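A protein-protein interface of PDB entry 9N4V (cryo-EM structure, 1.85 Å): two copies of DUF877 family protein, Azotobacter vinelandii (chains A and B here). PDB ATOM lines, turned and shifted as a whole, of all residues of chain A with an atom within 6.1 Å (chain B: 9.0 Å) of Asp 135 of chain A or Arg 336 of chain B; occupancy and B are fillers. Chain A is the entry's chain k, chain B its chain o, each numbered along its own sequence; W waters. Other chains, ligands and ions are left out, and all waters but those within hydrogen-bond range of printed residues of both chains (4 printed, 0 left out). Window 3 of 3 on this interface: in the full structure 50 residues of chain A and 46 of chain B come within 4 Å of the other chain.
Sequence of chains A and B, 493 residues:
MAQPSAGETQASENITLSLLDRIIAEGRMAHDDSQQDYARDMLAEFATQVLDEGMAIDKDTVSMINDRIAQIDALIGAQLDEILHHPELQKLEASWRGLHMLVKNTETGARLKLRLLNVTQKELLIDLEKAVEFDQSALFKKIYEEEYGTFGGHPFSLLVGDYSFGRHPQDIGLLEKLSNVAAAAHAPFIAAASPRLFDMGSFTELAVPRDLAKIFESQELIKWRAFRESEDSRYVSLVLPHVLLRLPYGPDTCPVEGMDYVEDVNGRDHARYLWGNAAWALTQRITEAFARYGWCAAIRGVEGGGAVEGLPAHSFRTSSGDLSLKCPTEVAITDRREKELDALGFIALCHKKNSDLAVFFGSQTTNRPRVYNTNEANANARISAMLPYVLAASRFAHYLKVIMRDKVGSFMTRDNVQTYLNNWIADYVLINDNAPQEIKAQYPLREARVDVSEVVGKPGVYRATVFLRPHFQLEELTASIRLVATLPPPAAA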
ATOM      1  N   GLU A 133     -20.713  -7.336   3.750  1.00  0.00           N
ATOM      2  CA  GLU A 133     -20.866  -7.552   5.181  1.00  0.00           C
ATOM      3  C   GLU A 133     -20.121  -8.828   5.545  1.00  0.00           C
ATOM      4  O   GLU A 133     -19.772  -9.625   4.675  1.00  0.00           O
ATOM      5  CB  GLU A 133     -22.345  -7.637   5.593  1.00  0.00           C
ATOM      6  CG  GLU A 133     -22.617  -7.198   7.025  1.00  0.00           C
ATOM      7  CD  GLU A 133     -24.098  -7.176   7.379  1.00  0.00           C
ATOM      8  OE1 GLU A 133     -24.914  -7.703   6.598  1.00  0.00           O
ATOM      9  OE2 GLU A 133     -24.443  -6.633   8.449  1.00  0.00           O
ATOM     10  N   PHE A 134     -19.863  -9.013   6.842  1.00  0.00           N
ATOM     11  CA  PHE A 134     -19.008 -10.124   7.254  1.00  0.00           C
ATOM     12  C   PHE A 134     -19.612 -11.477   6.892  1.00  0.00           C
ATOM     13  O   PHE A 134     -18.873 -12.434   6.649  1.00  0.00           O
ATOM     14  CB  PHE A 134     -18.699 -10.040   8.755  1.00  0.00           C
ATOM     15  CG  PHE A 134     -19.834 -10.453   9.643  1.00  0.00           C
ATOM     16  CD1 PHE A 134     -19.991 -11.776  10.027  1.00  0.00           C
ATOM     17  CD2 PHE A 134     -20.732  -9.512  10.116  1.00  0.00           C
ATOM     18  CE1 PHE A 134     -21.031 -12.153  10.843  1.00  0.00           C
ATOM     19  CE2 PHE A 134     -21.774  -9.887  10.937  1.00  0.00           C
ATOM     20  CZ  PHE A 134     -21.922 -11.208  11.301  1.00  0.00           C
ATOM     21  N   ASP A 135     -20.937 -11.582   6.841  1.00  0.00           N
ATOM     22  CA  ASP A 135     -21.571 -12.854   6.529  1.00  0.00           C
ATOM     23  C   ASP A 135     -21.817 -13.046   5.038  1.00  0.00           C
ATOM     24  O   ASP A 135     -22.464 -14.022   4.652  1.00  0.00           O
ATOM     25  CB  ASP A 135     -22.891 -13.009   7.295  1.00  0.00           C
ATOM     26  CG  ASP A 135     -23.910 -11.941   6.950  1.00  0.00           C
ATOM     27  OD1 ASP A 135     -23.583 -11.005   6.197  1.00  0.00           O
ATOM     28  OD2 ASP A 135     -25.056 -12.047   7.430  1.00  0.00           O
ATOM     29  N   GLN A 136     -21.327 -12.139   4.199  1.00  0.00           N
ATOM     30  CA  GLN A 136     -21.548 -12.211   2.763  1.00  0.00           C
ATOM     31  C   GLN A 136     -20.353 -12.754   1.990  1.00  0.00           C
ATOM     32  O   GLN A 136     -20.489 -13.029   0.795  1.00  0.00           O
ATOM     33  CB  GLN A 136     -21.924 -10.825   2.228  1.00  0.00           C
ATOM     34  CG  GLN A 136     -23.182 -10.265   2.865  1.00  0.00           C
ATOM     35  CD  GLN A 136     -24.359 -11.210   2.747  1.00  0.00           C
ATOM     36  OE1 GLN A 136     -24.766 -11.572   1.649  1.00  0.00           O
ATOM     37  NE2 GLN A 136     -24.912 -11.614   3.882  1.00  0.00           N
ATOM     38  N   SER A 137     -19.202 -12.919   2.633  1.00  0.00           N
ATOM     39  CA  SER A 137     -18.025 -13.426   1.942  1.00  0.00           C
ATOM     40  C   SER A 137     -18.229 -14.877   1.520  1.00  0.00           C
ATOM     41  O   SER A 137     -18.954 -15.639   2.162  1.00  0.00           O
ATOM     42  CB  SER A 137     -16.789 -13.310   2.833  1.00  0.00           C
ATOM     43  OG  SER A 137     -16.789 -14.293   3.852  1.00  0.00           O
ATOM     44  N   PHE A 140     -17.370 -17.182   4.300  1.00  0.00           N
ATOM     45  CA  PHE A 140     -18.408 -17.297   5.318  1.00  0.00           C
ATOM     46  C   PHE A 140     -19.536 -18.194   4.836  1.00  0.00           C
ATOM     47  O   PHE A 140     -19.969 -19.092   5.558  1.00  0.00           O
ATOM     48  CB  PHE A 140     -18.957 -15.929   5.720  1.00  0.00           C
ATOM     49  CG  PHE A 140     -19.901 -15.991   6.897  1.00  0.00           C
ATOM     50  CD1 PHE A 140     -21.244 -16.281   6.716  1.00  0.00           C
ATOM     51  CD2 PHE A 140     -19.437 -15.793   8.186  1.00  0.00           C
ATOM     52  CE1 PHE A 140     -22.108 -16.350   7.794  1.00  0.00           C
ATOM     53  CE2 PHE A 140     -20.294 -15.862   9.265  1.00  0.00           C
ATOM     54  CZ  PHE A 140     -21.632 -16.145   9.067  1.00  0.00           C
ATOM     55  N   LYS A 141     -20.006 -17.983   3.605  1.00  0.00           N
ATOM     56  CA  LYS A 141     -21.071 -18.831   3.080  1.00  0.00           C
ATOM     57  C   LYS A 141     -20.662 -20.299   3.130  1.00  0.00           C
ATOM     58  O   LYS A 141     -21.296 -21.101   3.822  1.00  0.00           O
ATOM     59  CB  LYS A 141     -21.427 -18.410   1.655  1.00  0.00           C
ATOM     60  CG  LYS A 141     -21.942 -16.989   1.554  1.00  0.00           C
ATOM     61  CD  LYS A 141     -23.421 -16.916   1.852  1.00  0.00           C
ATOM     62  CE  LYS A 141     -23.941 -15.493   1.737  1.00  0.00           C
ATOM     63  NZ  LYS A 141     -23.254 -14.759   0.640  1.00  0.00           N
ATOM     64  N   TYR A 144     -19.571 -21.387   7.183  1.00  0.00           N
ATOM     65  CA  TYR A 144     -20.644 -21.275   8.158  1.00  0.00           C
ATOM     66  C   TYR A 144     -21.980 -21.723   7.576  1.00  0.00           C
ATOM     67  O   TYR A 144     -22.573 -22.695   8.050  1.00  0.00           O
ATOM     68  CB  TYR A 144     -20.732 -19.830   8.665  1.00  0.00           C
ATOM     69  CG  TYR A 144     -21.791 -19.591   9.717  1.00  0.00           C
ATOM     70  CD1 TYR A 144     -23.117 -19.378   9.363  1.00  0.00           C
ATOM     71  CD2 TYR A 144     -21.460 -19.558  11.066  1.00  0.00           C
ATOM     72  CE1 TYR A 144     -24.085 -19.154  10.319  1.00  0.00           C
ATOM     73  CE2 TYR A 144     -22.420 -19.333  12.028  1.00  0.00           C
ATOM     74  CZ  TYR A 144     -23.732 -19.133  11.650  1.00  0.00           C
ATOM     75  OH  TYR A 144     -24.690 -18.909  12.605  1.00  0.00           O
ATOM     76  N   GLU A 145     -22.464 -21.031   6.539  1.00  0.00           N
ATOM     77  CA  GLU A 145     -23.869 -21.176   6.175  1.00  0.00           C
ATOM     78  C   GLU A 145     -24.155 -22.558   5.610  1.00  0.00           C
ATOM     79  O   GLU A 145     -25.134 -23.201   5.997  1.00  0.00           O
ATOM     80  CB  GLU A 145     -24.278 -20.095   5.171  1.00  0.00           C
ATOM     81  CG  GLU A 145     -24.160 -18.665   5.688  1.00  0.00           C
ATOM     82  CD  GLU A 145     -25.348 -18.235   6.536  1.00  0.00           C
ATOM     83  OE1 GLU A 145     -25.954 -19.087   7.213  1.00  0.00           O
ATOM     84  OE2 GLU A 145     -25.676 -17.035   6.527  1.00  0.00           O
ATOM     85  N   GLY A 149     -24.705 -23.802   9.427  1.00  0.00           N
ATOM     86  CA  GLY A 149     -25.962 -23.087   9.464  1.00  0.00           C
ATOM     87  C   GLY A 149     -27.056 -23.629   8.564  1.00  0.00           C
ATOM     88  O   GLY A 149     -27.989 -22.899   8.233  1.00  0.00           O
ATOM     89  N   ALA B 207     -32.147 -17.088  -1.546  1.00  0.00           N
ATOM     90  CA  ALA B 207     -30.903 -16.921  -0.805  1.00  0.00           C
ATOM     91  C   ALA B 207     -30.089 -15.717  -1.263  1.00  0.00           C
ATOM     92  O   ALA B 207     -29.071 -15.411  -0.641  1.00  0.00           O
ATOM     93  CB  ALA B 207     -30.054 -18.190  -0.910  1.00  0.00           C
ATOM     94  N   PRO B 209     -30.835 -12.120  -1.582  1.00  0.00           N
ATOM     95  CA  PRO B 209     -30.775 -10.865  -0.819  1.00  0.00           C
ATOM     96  C   PRO B 209     -29.994 -11.022   0.478  1.00  0.00           C
ATOM     97  O   PRO B 209     -30.073 -12.052   1.149  1.00  0.00           O
ATOM     98  CB  PRO B 209     -32.249 -10.545  -0.547  1.00  0.00           C
ATOM     99  CG  PRO B 209     -32.998 -11.311  -1.558  1.00  0.00           C
ATOM    100  CD  PRO B 209     -32.229 -12.569  -1.743  1.00  0.00           C
ATOM    101  N   ARG B 210     -29.222  -9.987   0.820  1.00  0.00           N
ATOM    102  CA  ARG B 210     -28.509  -9.998   2.094  1.00  0.00           C
ATOM    103  C   ARG B 210     -29.476  -9.970   3.271  1.00  0.00           C
ATOM    104  O   ARG B 210     -29.304 -10.717   4.239  1.00  0.00           O
ATOM    105  CB  ARG B 210     -27.540  -8.819   2.175  1.00  0.00           C
ATOM    106  CG  ARG B 210     -26.879  -8.651   3.537  1.00  0.00           C
ATOM    107  CD  ARG B 210     -25.976  -7.428   3.575  1.00  0.00           C
ATOM    108  NE  ARG B 210     -26.728  -6.192   3.406  1.00  0.00           N
ATOM    109  CZ  ARG B 210     -27.373  -5.564   4.379  1.00  0.00           C
ATOM    110  NH1 ARG B 210     -27.352  -6.011   5.622  1.00  0.00           N
ATOM    111  NH2 ARG B 210     -28.059  -4.462   4.095  1.00  0.00           N
ATOM    112  N   ASP B 211     -30.501  -9.122   3.203  1.00  0.00           N
ATOM    113  CA  ASP B 211     -31.436  -8.927   4.308  1.00  0.00           C
ATOM    114  C   ASP B 211     -32.862  -8.972   3.775  1.00  0.00           C
ATOM    115  O   ASP B 211     -33.280  -8.082   3.030  1.00  0.00           O
ATOM    116  CB  ASP B 211     -31.162  -7.607   5.028  1.00  0.00           C
ATOM    117  CG  ASP B 211     -31.981  -7.455   6.290  1.00  0.00           C
ATOM    118  OD1 ASP B 211     -31.698  -8.167   7.276  1.00  0.00           O
ATOM    119  OD2 ASP B 211     -32.904  -6.620   6.300  1.00  0.00           O
ATOM    120  N   LEU B 212     -33.611 -10.002   4.174  1.00  0.00           N
ATOM    121  CA  LEU B 212     -34.988 -10.154   3.714  1.00  0.00           C
ATOM    122  C   LEU B 212     -35.886  -9.041   4.241  1.00  0.00           C
ATOM    123  O   LEU B 212     -36.747  -8.537   3.514  1.00  0.00           O
ATOM    124  CB  LEU B 212     -35.536 -11.513   4.145  1.00  0.00           C
ATOM    125  CG  LEU B 212     -35.103 -12.760   3.380  1.00  0.00           C
ATOM    126  CD1 LEU B 212     -36.049 -13.892   3.711  1.00  0.00           C
ATOM    127  CD2 LEU B 212     -35.069 -12.508   1.884  1.00  0.00           C
ATOM    128  N   ILE B 333     -32.778 -23.436   2.537  1.00  0.00           N
ATOM    129  CA  ILE B 333     -33.057 -22.332   3.444  1.00  0.00           C
ATOM    130  C   ILE B 333     -32.211 -22.542   4.692  1.00  0.00           C
ATOM    131  O   ILE B 333     -32.439 -23.489   5.452  1.00  0.00           O
ATOM    132  CB  ILE B 333     -34.550 -22.240   3.784  1.00  0.00           C
ATOM    133  CG1 ILE B 333     -35.358 -21.969   2.509  1.00  0.00           C
ATOM    134  CG2 ILE B 333     -34.802 -21.173   4.849  1.00  0.00           C
ATOM    135  CD1 ILE B 333     -36.842 -21.936   2.718  1.00  0.00           C
ATOM    136  N   THR B 334     -31.236 -21.663   4.902  1.00  0.00           N
ATOM    137  CA  THR B 334     -30.391 -21.746   6.082  1.00  0.00           C
ATOM    138  C   THR B 334     -31.209 -21.452   7.342  1.00  0.00           C
ATOM    139  O   THR B 334     -32.329 -20.940   7.286  1.00  0.00           O
ATOM    140  CB  THR B 334     -29.213 -20.774   5.972  1.00  0.00           C
ATOM    141  OG1 THR B 334     -29.693 -19.426   6.031  1.00  0.00           O
ATOM    142  CG2 THR B 334     -28.461 -20.979   4.663  1.00  0.00           C
ATOM    143  N   ASP B 335     -30.632 -21.801   8.496  1.00  0.00           N
ATOM    144  CA  ASP B 335     -31.285 -21.517   9.771  1.00  0.00           C
ATOM    145  C   ASP B 335     -31.571 -20.028   9.923  1.00  0.00           C
ATOM    146  O   ASP B 335     -32.677 -19.634  10.318  1.00  0.00           O
ATOM    147  CB  ASP B 335     -30.416 -22.004  10.932  1.00  0.00           C
ATOM    148  CG  ASP B 335     -30.436 -23.514  11.094  1.00  0.00           C
ATOM    149  OD1 ASP B 335     -31.139 -24.199  10.324  1.00  0.00           O
ATOM    150  OD2 ASP B 335     -29.747 -24.018  12.004  1.00  0.00           O
ATOM    151  N   ARG B 336     -30.587 -19.185   9.606  1.00  0.00           N
ATOM    152  CA  ARG B 336     -30.773 -17.745   9.734  1.00  0.00           C
ATOM    153  C   ARG B 336     -31.876 -17.253   8.807  1.00  0.00           C
ATOM    154  O   ARG B 336     -32.691 -16.406   9.191  1.00  0.00           O
ATOM    155  CB  ARG B 336     -29.457 -17.022   9.447  1.00  0.00           C
ATOM    156  CG  ARG B 336     -28.378 -17.265  10.494  1.00  0.00           C
ATOM    157  CD  ARG B 336     -27.035 -16.712  10.064  1.00  0.00           C
ATOM    158  NE  ARG B 336     -26.952 -15.270  10.257  1.00  0.00           N
ATOM    159  CZ  ARG B 336     -26.282 -14.441   9.469  1.00  0.00           C
ATOM    160  NH1 ARG B 336     -25.624 -14.875   8.407  1.00  0.00           N
ATOM    161  NH2 ARG B 336     -26.278 -13.144   9.751  1.00  0.00           N
ATOM    162  N   ARG B 337     -31.919 -17.782   7.584  1.00  0.00           N
ATOM    163  CA  ARG B 337     -32.950 -17.386   6.630  1.00  0.00           C
ATOM    164  C   ARG B 337     -34.330 -17.846   7.079  1.00  0.00           C
ATOM    165  O   ARG B 337     -35.315 -17.113   6.928  1.00  0.00           O
ATOM    166  CB  ARG B 337     -32.629 -17.948   5.250  1.00  0.00           C
ATOM    167  CG  ARG B 337     -33.485 -17.358   4.164  1.00  0.00           C
ATOM    168  CD  ARG B 337     -33.200 -15.886   4.054  1.00  0.00           C
ATOM    169  NE  ARG B 337     -32.479 -15.565   2.836  1.00  0.00           N
ATOM    170  CZ  ARG B 337     -31.736 -14.482   2.664  1.00  0.00           C
ATOM    171  NH1 ARG B 337     -31.552 -13.606   3.637  1.00  0.00           N
ATOM    172  NH2 ARG B 337     -31.160 -14.275   1.488  1.00  0.00           N
ATOM    173  N   GLU B 338     -34.425 -19.062   7.619  1.00  0.00           N
ATOM    174  CA  GLU B 338     -35.701 -19.525   8.148  1.00  0.00           C
ATOM    175  C   GLU B 338     -36.181 -18.621   9.273  1.00  0.00           C
ATOM    176  O   GLU B 338     -37.371 -18.307   9.357  1.00  0.00           O
ATOM    177  CB  GLU B 338     -35.594 -20.974   8.633  1.00  0.00           C
ATOM    178  CG  GLU B 338     -36.944 -21.590   8.990  1.00  0.00           C
ATOM    179  CD  GLU B 338     -37.390 -21.264  10.409  1.00  0.00           C
ATOM    180  OE1 GLU B 338     -36.524 -21.012  11.266  1.00  0.00           O
ATOM    181  OE2 GLU B 338     -38.609 -21.228  10.658  1.00  0.00           O
ATOM    182  N   LYS B 339     -35.268 -18.198  10.152  1.00  0.00           N
ATOM    183  CA  LYS B 339     -35.660 -17.305  11.239  1.00  0.00           C
ATOM    184  C   LYS B 339     -36.115 -15.946  10.714  1.00  0.00           C
ATOM    185  O   LYS B 339     -37.106 -15.389  11.201  1.00  0.00           O
ATOM    186  CB  LYS B 339     -34.513 -17.141  12.234  1.00  0.00           C
ATOM    187  CG  LYS B 339     -34.953 -16.592  13.582  1.00  0.00           C
ATOM    188  CD  LYS B 339     -36.237 -17.252  14.046  1.00  0.00           C
ATOM    189  CE  LYS B 339     -36.610 -16.849  15.463  1.00  0.00           C
ATOM    190  NZ  LYS B 339     -36.216 -15.453  15.786  1.00  0.00           N
ATOM    191  N   GLU B 340     -35.405 -15.399   9.720  1.00  0.00           N
ATOM    192  CA  GLU B 340     -35.863 -14.170   9.069  1.00  0.00           C
ATOM    193  C   GLU B 340     -37.282 -14.329   8.540  1.00  0.00           C
ATOM    194  O   GLU B 340     -38.149 -13.486   8.790  1.00  0.00           O
ATOM    195  CB  GLU B 340     -34.944 -13.787   7.909  1.00  0.00           C
ATOM    196  CG  GLU B 340     -33.532 -13.408   8.232  1.00  0.00           C
ATOM    197  CD  GLU B 340     -32.773 -13.039   6.970  1.00  0.00           C
ATOM    198  OE1 GLU B 340     -33.023 -11.947   6.423  1.00  0.00           O
ATOM    199  OE2 GLU B 340     -31.957 -13.856   6.503  1.00  0.00           O
ATOM    200  N   LEU B 341     -37.525 -15.403   7.786  1.00  0.00           N
ATOM    201  CA  LEU B 341     -38.841 -15.619   7.196  1.00  0.00           C
ATOM    202  C   LEU B 341     -39.911 -15.751   8.270  1.00  0.00           C
ATOM    203  O   LEU B 341     -41.014 -15.215   8.124  1.00  0.00           O
ATOM    204  CB  LEU B 341     -38.821 -16.863   6.317  1.00  0.00           C
ATOM    205  CG  LEU B 341     -38.086 -16.717   4.990  1.00  0.00           C
ATOM    206  CD1 LEU B 341     -37.733 -18.083   4.434  1.00  0.00           C
ATOM    207  CD2 LEU B 341     -38.937 -15.923   4.009  1.00  0.00           C
ATOM    208  N   ASP B 342     -39.601 -16.467   9.349  1.00  0.00           N
ATOM    209  CA  ASP B 342     -40.538 -16.580  10.458  1.00  0.00           C
ATOM    210  C   ASP B 342     -40.872 -15.207  11.025  1.00  0.00           C
ATOM    211  O   ASP B 342     -42.037 -14.914  11.308  1.00  0.00           O
ATOM    212  CB  ASP B 342     -39.950 -17.493  11.536  1.00  0.00           C
ATOM    213  CG  ASP B 342     -40.821 -17.582  12.770  1.00  0.00           C
ATOM    214  OD1 ASP B 342     -40.695 -16.712  13.652  1.00  0.00           O
ATOM    215  OD2 ASP B 342     -41.625 -18.528  12.865  1.00  0.00           O
ATOM    216  N   ALA B 343     -39.862 -14.346  11.178  1.00  0.00           N
ATOM    217  CA  ALA B 343     -40.110 -13.001  11.687  1.00  0.00           C
ATOM    218  C   ALA B 343     -40.969 -12.180  10.735  1.00  0.00           C
ATOM    219  O   ALA B 343     -41.679 -11.270  11.169  1.00  0.00           O
ATOM    220  CB  ALA B 343     -38.786 -12.281  11.947  1.00  0.00           C
ATOM    221  N   LEU B 344     -40.927 -12.481   9.443  1.00  0.00           N
ATOM    222  CA  LEU B 344     -41.678 -11.717   8.458  1.00  0.00           C
ATOM    223  C   LEU B 344     -43.089 -12.253   8.242  1.00  0.00           C
ATOM    224  O   LEU B 344     -43.818 -11.716   7.406  1.00  0.00           O
ATOM    225  CB  LEU B 344     -40.911 -11.677   7.134  1.00  0.00           C
ATOM    226  CG  LEU B 344     -39.616 -10.861   7.217  1.00  0.00           C
ATOM    227  CD1 LEU B 344     -38.685 -11.160   6.050  1.00  0.00           C
ATOM    228  CD2 LEU B 344     -39.929  -9.379   7.291  1.00  0.00           C
ATOM    229  N   CYS B 350     -38.104 -26.357   4.939  1.00  0.00           N
ATOM    230  CA  CYS B 350     -36.646 -26.395   4.891  1.00  0.00           C
ATOM    231  C   CYS B 350     -36.159 -27.801   4.561  1.00  0.00           C
ATOM    232  O   CYS B 350     -36.332 -28.724   5.361  1.00  0.00           O
ATOM    233  CB  CYS B 350     -36.051 -25.933   6.219  1.00  0.00           C
ATOM    234  SG  CYS B 350     -36.530 -24.262   6.688  1.00  0.00           S
HETATM  235  O   HOH W   1     -28.213 -17.175   5.826  1.00  0.00           O
HETATM  236  O   HOH W   2     -27.032  -6.094   8.575  1.00  0.00           O
HETATM  237  O   HOH W   3     -27.631 -20.330   9.123  1.00  0.00           O
HETATM  238  O   HOH W   4     -27.570 -13.483   5.864  1.00  0.00           O
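The side-chain hydroxyl (OG1) of Thr 334 of chain B is in hydrogen-bond range of the backbone NH (N) of Arg 337 of chain B (3.2 Å). The side-chain carboxylate (OD1) of Asp 135 of chain A lies within hydrogen-bond range of the side-chain amide nitrogen (NE2) of Gln 136 of chain A (2.7 Å). NZ of Lys 141 of chain A is in hydrogen-bond range of O of Gln 136 of chain A (3.3 Å). The backbone carbonyl oxygen of Tyr 144 of chain A lies within hydrogen-bond range of the backbone NH of Gly 149 of chain A, at 2.8 Å. The side-chain hydroxyl (OG) of Ser 137 of chain A sits at hydrogen-bond distance from the backbone NH (N) of Phe 140 of chain A, at 3.0 Å. The backbone carbonyl oxygen (O) of Phe 140 of chain A is in hydrogen-bond range of the backbone NH (N) of Glu 145 of chain A (3.3 Å).
Printed residues of chain A that touch a printed residue of chain B: Glu 133, Asp 135, Gln 136, Phe 140, Tyr 144, Glu 145 and Gly 149. Among the printed residues, 9 pairs touch across the chains. Among the printed residues, Asp or Glu carboxylates within 4 Å of a Lys or Arg side-chain nitrogen of the other chain: Glu 133 of chain A with Arg 210 of chain B (3.1 Å), Asp 135 of chain A with Arg 336 of chain B (2.8 Å) and Glu 145 of chain A with Arg 336 of chain B (2.9 Å).
Of chain A, only Asp 135 (2.8 Å), Phe 140 (3.9 Å), Tyr 144 (3.8 Å) and Glu 145 (2.9 Å) come within 4 Å of Arg 336 of chain B. Of chain B, only Arg 210 comes within 4 Å of Gln 136 of chain A. Printed residues of chain A within 4 Å of Arg 210 of chain B: Glu 133 (3.1 Å) and Gln 136 (3.6 Å). Of the printed residues of chain A, Thr 334 of chain B touches Glu 145 and Gly 149. Printed residues of chain B within 4 Å of Glu 133 of chain A: Arg 210. Of the printed residues of chain B, Gly 149 of chain A touches Thr 334 and Asp 335. Printed residues of chain B within 4 Å of Phe 140 of chain A: Arg 336 (3.9 Å). The nearest residue of chain B that does not touch Asp 135 of chain A is Arg 210 of chain B (4.8 Å). The nearest residue of chain A that does not touch Arg 336 of chain B is Gly 149 of chain A (4.7 Å). The nearest printed residue of chain B that does not touch Glu 133 of chain A is Arg 336 of chain B (6.4 Å).
No position is printed for both chains. Of the 9 pairs that touch across the chains among the printed residues, none has its exchanged pair printed and touching as well.
Among the printed residues, pairs that only touch across the chains: Gln 136 of chain A with Arg 210 of chain B (3.6 Å), Phe 140 of chain A with Arg 336 of chain B (3.9 Å), Tyr 144 of chain A with Arg 336 of chain B (3.8 Å), Glu 145 of chain A with Thr 334 of chain B (3.9 Å) and Gly 149 of chain A with Thr 334 of chain B (3.3 Å).
Water W1 lies within hydrogen-bond range of OE2 of Glu 145 of chain A and OG1 of Thr 334 of chain B. Water W2 bridges OE2 of Glu 133 of chain A (2.6 Å) and NH1 of Arg 210 of chain B (3.0 Å). Water W3 lies within hydrogen-bond range of O of Gly 149 of chain A (2.7 Å), OE1 of Glu 145 of chain A (2.8 Å), N of Arg 336 of chain B (3.2 Å) and N of Asp 335 of chain B (3.4 Å). Water W4 bridges the side-chain carboxylate (OD2) of Asp 135 of chain A (3.3 Å) and the guanidinium group (NH1) of Arg 336 of chain B (3.5 Å).
The side-chain carboxylate (OE1) of Glu 133 of chain A lies within salt-bridge range of the guanidinium group (NH1) of Arg 210 of chain B (3.1 Å). The side-chain carboxylate of Glu 145 of chain A lies within salt-bridge range of the guanidinium group of Arg 336 of chain B (2.9 Å). OD2 of Asp 135 of chain A is in salt-bridge range of NH2 of Arg 336 of chain B (2.8 Å). O of Gly 149 of chain A lies within hydrogen-bond range of N of Asp 335 of chain B (2.9 Å).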
